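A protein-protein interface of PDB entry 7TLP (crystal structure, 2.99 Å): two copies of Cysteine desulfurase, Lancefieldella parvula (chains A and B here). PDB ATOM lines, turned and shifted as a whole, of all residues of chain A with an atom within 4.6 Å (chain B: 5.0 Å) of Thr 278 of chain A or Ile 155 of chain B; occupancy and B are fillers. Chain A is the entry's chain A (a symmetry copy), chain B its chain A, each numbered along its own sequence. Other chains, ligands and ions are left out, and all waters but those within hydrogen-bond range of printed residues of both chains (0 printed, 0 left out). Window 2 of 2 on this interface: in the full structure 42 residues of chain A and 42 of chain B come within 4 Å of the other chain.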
ATOM      1  N   PHE A 276      15.530 -20.824  19.311  1.00  0.00           N
ATOM      2  CA  PHE A 276      16.460 -20.976  18.197  1.00  0.00           C
ATOM      3  C   PHE A 276      17.270 -22.218  18.529  1.00  0.00           C
ATOM      4  O   PHE A 276      16.892 -23.314  18.118  1.00  0.00           O
ATOM      5  CB  PHE A 276      17.292 -19.682  17.987  1.00  0.00           C
ATOM      6  CG  PHE A 276      18.468 -19.833  17.050  1.00  0.00           C
ATOM      7  CD1 PHE A 276      18.297 -20.301  15.766  1.00  0.00           C
ATOM      8  CD2 PHE A 276      19.761 -19.559  17.496  1.00  0.00           C
ATOM      9  CE1 PHE A 276      19.379 -20.472  14.942  1.00  0.00           C
ATOM     10  CE2 PHE A 276      20.838 -19.751  16.682  1.00  0.00           C
ATOM     11  CZ  PHE A 276      20.648 -20.207  15.403  1.00  0.00           C
ATOM     12  N   LEU A 277      18.314 -22.099  19.337  1.00  0.00           N
ATOM     13  CA  LEU A 277      18.985 -23.305  19.815  1.00  0.00           C
ATOM     14  C   LEU A 277      18.129 -24.061  20.833  1.00  0.00           C
ATOM     15  O   LEU A 277      17.453 -23.452  21.675  1.00  0.00           O
ATOM     16  CB  LEU A 277      20.325 -22.969  20.451  1.00  0.00           C
ATOM     17  CG  LEU A 277      21.419 -22.497  19.550  1.00  0.00           C
ATOM     18  CD1 LEU A 277      22.708 -22.844  20.234  1.00  0.00           C
ATOM     19  CD2 LEU A 277      21.324 -23.172  18.212  1.00  0.00           C
ATOM     20  N   THR A 278      18.210 -25.392  20.787  1.00  0.00           N
ATOM     21  CA  THR A 278      17.419 -26.260  21.652  1.00  0.00           C
ATOM     22  C   THR A 278      18.315 -27.218  22.427  1.00  0.00           C
ATOM     23  O   THR A 278      19.416 -27.573  21.995  1.00  0.00           O
ATOM     24  CB  THR A 278      16.371 -27.077  20.873  1.00  0.00           C
ATOM     25  OG1 THR A 278      16.990 -27.732  19.756  1.00  0.00           O
ATOM     26  CG2 THR A 278      15.267 -26.156  20.349  1.00  0.00           C
ATOM     27  N   GLY A 279      17.827 -27.649  23.568  1.00  0.00           N
ATOM     28  CA  GLY A 279      18.467 -28.721  24.264  1.00  0.00           C
ATOM     29  C   GLY A 279      18.193 -28.607  25.752  1.00  0.00           C
ATOM     30  O   GLY A 279      17.059 -28.330  26.152  1.00  0.00           O
ATOM     31  N   GLY A 280      19.246 -28.818  26.540  1.00  0.00           N
ATOM     32  CA  GLY A 280      19.147 -28.723  27.980  1.00  0.00           C
ATOM     33  C   GLY A 280      19.322 -27.295  28.476  1.00  0.00           C
ATOM     34  O   GLY A 280      20.271 -26.606  28.093  1.00  0.00           O
ATOM     35  N   MET A 282      17.612 -24.421  28.035  1.00  0.00           N
ATOM     36  CA  MET A 282      16.351 -24.395  27.362  1.00  0.00           C
ATOM     37  C   MET A 282      15.445 -25.630  27.658  1.00  0.00           C
ATOM     38  O   MET A 282      14.873 -25.666  28.761  1.00  0.00           O
ATOM     39  CB  MET A 282      16.485 -24.171  25.828  1.00  0.00           C
ATOM     40  CG  MET A 282      14.936 -24.271  25.540  1.00  0.00           C
ATOM     41  SD  MET A 282      14.324 -25.973  24.814  1.00  0.00           S
ATOM     42  CE  MET A 282      14.638 -25.161  23.103  1.00  0.00           C
ATOM     43  N   ALA A 302      20.805 -22.251  25.636  1.00  0.00           N
ATOM     44  CA  ALA A 302      20.931 -23.704  25.708  1.00  0.00           C
ATOM     45  C   ALA A 302      22.330 -24.103  26.179  1.00  0.00           C
ATOM     46  O   ALA A 302      23.338 -23.770  25.533  1.00  0.00           O
ATOM     47  CB  ALA A 302      20.635 -24.334  24.346  1.00  0.00           C
ATOM     48  N   SER B 122      26.107 -28.425  23.841  1.00  0.00           N
ATOM     49  CA  SER B 122      24.781 -28.208  23.309  1.00  0.00           C
ATOM     50  C   SER B 122      24.842 -27.530  21.959  1.00  0.00           C
ATOM     51  O   SER B 122      24.105 -27.896  21.043  1.00  0.00           O
ATOM     52  CB  SER B 122      23.986 -27.349  24.281  1.00  0.00           C
ATOM     53  OG  SER B 122      23.750 -28.022  25.506  1.00  0.00           O
ATOM     54  N   ASN B 126      23.560 -28.980  18.430  1.00  0.00           N
ATOM     55  CA  ASN B 126      22.620 -28.230  17.594  1.00  0.00           C
ATOM     56  C   ASN B 126      23.138 -28.037  16.163  1.00  0.00           C
ATOM     57  O   ASN B 126      22.374 -28.163  15.201  1.00  0.00           O
ATOM     58  CB  ASN B 126      22.336 -26.876  18.241  1.00  0.00           C
ATOM     59  CG  ASN B 126      21.109 -26.899  19.074  1.00  0.00           C
ATOM     60  OD1 ASN B 126      20.020 -26.722  18.577  1.00  0.00           O
ATOM     61  ND2 ASN B 126      21.271 -27.131  20.354  1.00  0.00           N
ATOM     62  N   HIS B 151      19.358 -34.018  27.130  1.00  0.00           N
ATOM     63  CA  HIS B 151      18.349 -33.367  26.282  1.00  0.00           C
ATOM     64  C   HIS B 151      18.981 -32.724  25.041  1.00  0.00           C
ATOM     65  O   HIS B 151      18.373 -32.702  23.964  1.00  0.00           O
ATOM     66  CB  HIS B 151      17.557 -32.322  27.098  1.00  0.00           C
ATOM     67  CG  HIS B 151      16.638 -32.906  28.148  1.00  0.00           C
ATOM     68  ND1 HIS B 151      16.083 -32.145  29.165  1.00  0.00           N
ATOM     69  CD2 HIS B 151      16.172 -34.172  28.336  1.00  0.00           C
ATOM     70  CE1 HIS B 151      15.330 -32.920  29.935  1.00  0.00           C
ATOM     71  NE2 HIS B 151      15.349 -34.147  29.442  1.00  0.00           N
ATOM     72  N   SER B 152      20.221 -32.228  25.165  1.00  0.00           N
ATOM     73  CA  SER B 152      20.903 -31.570  24.051  1.00  0.00           C
ATOM     74  C   SER B 152      21.202 -32.514  22.903  1.00  0.00           C
ATOM     75  O   SER B 152      21.451 -32.048  21.794  1.00  0.00           O
ATOM     76  CB  SER B 152      22.203 -30.939  24.518  1.00  0.00           C
ATOM     77  OG  SER B 152      21.939 -29.780  25.265  1.00  0.00           O
ATOM     78  N   ASN B 153      21.207 -33.823  23.149  1.00  0.00           N
ATOM     79  CA  ASN B 153      21.294 -34.834  22.110  1.00  0.00           C
ATOM     80  C   ASN B 153      19.928 -35.461  21.795  1.00  0.00           C
ATOM     81  O   ASN B 153      19.861 -36.562  21.247  1.00  0.00           O
ATOM     82  CB  ASN B 153      22.311 -35.892  22.525  1.00  0.00           C
ATOM     83  CG  ASN B 153      22.808 -36.717  21.361  1.00  0.00           C
ATOM     84  OD1 ASN B 153      22.735 -36.309  20.212  1.00  0.00           O
ATOM     85  ND2 ASN B 153      23.291 -37.911  21.657  1.00  0.00           N
ATOM     86  N   ILE B 154      18.829 -34.764  22.104  1.00  0.00           N
ATOM     87  CA  ILE B 154      17.483 -35.260  21.836  1.00  0.00           C
ATOM     88  C   ILE B 154      16.664 -34.251  21.061  1.00  0.00           C
ATOM     89  O   ILE B 154      16.182 -34.533  19.964  1.00  0.00           O
ATOM     90  CB  ILE B 154      16.713 -35.604  23.108  1.00  0.00           C
ATOM     91  CG1 ILE B 154      17.425 -36.727  23.864  1.00  0.00           C
ATOM     92  CG2 ILE B 154      15.291 -35.985  22.701  1.00  0.00           C
ATOM     93  CD1 ILE B 154      16.880 -36.978  25.200  1.00  0.00           C
ATOM     94  N   ILE B 155      16.466 -33.077  21.642  1.00  0.00           N
ATOM     95  CA  ILE B 155      15.548 -32.104  21.040  1.00  0.00           C
ATOM     96  C   ILE B 155      15.984 -31.642  19.656  1.00  0.00           C
ATOM     97  O   ILE B 155      15.127 -31.580  18.758  1.00  0.00           O
ATOM     98  CB  ILE B 155      15.326 -30.925  21.997  1.00  0.00           C
ATOM     99  CG1 ILE B 155      14.724 -31.452  23.292  1.00  0.00           C
ATOM    100  CG2 ILE B 155      14.385 -29.983  21.357  1.00  0.00           C
ATOM    101  CD1 ILE B 155      15.096 -30.621  24.497  1.00  0.00           C
ATOM    102  N   PRO B 156      17.244 -31.295  19.407  1.00  0.00           N
ATOM    103  CA  PRO B 156      17.599 -30.907  18.042  1.00  0.00           C
ATOM    104  C   PRO B 156      17.264 -31.978  17.036  1.00  0.00           C
ATOM    105  O   PRO B 156      16.826 -31.658  15.929  1.00  0.00           O
ATOM    106  CB  PRO B 156      19.102 -30.648  18.131  1.00  0.00           C
ATOM    107  CG  PRO B 156      19.297 -30.244  19.536  1.00  0.00           C
ATOM    108  CD  PRO B 156      18.370 -31.092  20.328  1.00  0.00           C
ATOM    109  N   TRP B 157      17.410 -33.247  17.410  1.00  0.00           N
ATOM    110  CA  TRP B 157      17.074 -34.348  16.512  1.00  0.00           C
ATOM    111  C   TRP B 157      15.581 -34.459  16.302  1.00  0.00           C
ATOM    112  O   TRP B 157      15.123 -34.882  15.237  1.00  0.00           O
ATOM    113  CB  TRP B 157      17.617 -35.644  17.075  1.00  0.00           C
ATOM    114  CG  TRP B 157      19.088 -35.619  17.121  1.00  0.00           C
ATOM    115  CD1 TRP B 157      19.866 -35.744  18.224  1.00  0.00           C
ATOM    116  CD2 TRP B 157      19.978 -35.471  16.007  1.00  0.00           C
ATOM    117  NE1 TRP B 157      21.188 -35.680  17.871  1.00  0.00           N
ATOM    118  CE2 TRP B 157      21.283 -35.514  16.515  1.00  0.00           C
ATOM    119  CE3 TRP B 157      19.797 -35.321  14.638  1.00  0.00           C
ATOM    120  CZ2 TRP B 157      22.403 -35.398  15.704  1.00  0.00           C
ATOM    121  CZ3 TRP B 157      20.909 -35.208  13.840  1.00  0.00           C
ATOM    122  CH2 TRP B 157      22.192 -35.240  14.376  1.00  0.00           C
ATOM    123  N   GLN B 158      14.808 -34.089  17.310  1.00  0.00           N
ATOM    124  CA  GLN B 158      13.368 -34.067  17.145  1.00  0.00           C
ATOM    125  C   GLN B 158      12.971 -33.019  16.125  1.00  0.00           C
ATOM    126  O   GLN B 158      12.169 -33.291  15.223  1.00  0.00           O
ATOM    127  CB  GLN B 158      12.712 -33.820  18.491  1.00  0.00           C
ATOM    128  CG  GLN B 158      12.596 -35.056  19.301  1.00  0.00           C
ATOM    129  CD  GLN B 158      12.037 -34.762  20.658  1.00  0.00           C
ATOM    130  OE1 GLN B 158      12.433 -33.801  21.299  1.00  0.00           O
ATOM    131  NE2 GLN B 158      11.065 -35.556  21.088  1.00  0.00           N
ATOM    132  N   GLN B 159      13.547 -31.821  16.234  1.00  0.00           N
ATOM    133  CA  GLN B 159      13.291 -30.790  15.237  1.00  0.00           C
ATOM    134  C   GLN B 159      13.732 -31.261  13.855  1.00  0.00           C
ATOM    135  O   GLN B 159      12.927 -31.324  12.926  1.00  0.00           O
ATOM    136  CB  GLN B 159      13.986 -29.490  15.647  1.00  0.00           C
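Of the printed residues of chain B, Leu 277 of chain A touches Asn 126. Thr 278 of chain A touches just these residues of chain B: Asn 126 (2.5 Å), Ile 155 (3.6 Å) and Pro 156 (3.4 Å). Of the printed residues of chain B, Gly 280 of chain A touches His 151 and Ser 152. Of the printed residues of chain A, Asn 126 of chain B touches Leu 277 (3.8 Å) and Thr 278 (2.5 Å). Ile 155 of chain B touches just these residues of chain A: Thr 278 and Gly 279. The nearest residue of chain B that does not touch Thr 278 of chain A is Ser 152 of chain B (4.7 Å).
ND2 of Asn 126 of chain B is in hydrogen-bond range of O of Thr 278 of chain A, 2.5 Å away. The side-chain hydroxyl (OG) of Ser 152 of chain B is in hydrogen-bond range of the backbone NH (N) of Gly 280 of chain A (3.1 Å).
Along chain B the printed residues that touch a printed residue of chain A span positions 122 to 156. Hydrophobic or aromatic side chains of chain A within 4 Å of the printed part of chain B: Leu 277. Among the printed residues, 10 pairs touch across the chains.
Leu 277 of chain A touches Asn 126 of chain B (CA to OD1, 3.8 Å). Thr 278 of chain A touches Ile 155 of chain B (CB to CG2, 3.6 Å). Thr 278 of chain A touches Pro 156 of chain B. O of His 151 of chain B touches CA of Gly 279 of chain A, 3.99 Å away. Gly 279 of chain A touches Ser 152 of chain B. Ile 155 of chain B touches Gly 279 of chain A (CD1 to O, 3.4 Å). Gly 280 of chain A touches His 151 of chain B. Ser 122 of chain B touches Ala 302 of chain A (CB to O, 3.8 Å).
No position is printed for both chains. Of the 10 pairs that touch across the chains among the printed residues, none has its exchanged pair printed and touching as well.
ND2 of Asn 126 of chain B sits at hydrogen-bond distance from O of Ser 122 of chain B (3.0 Å). The side-chain hydroxyl (OG) of Ser 122 of chain B is in hydrogen-bond range of the side-chain hydroxyl (OG) of Ser 152 of chain B (2.5 Å).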
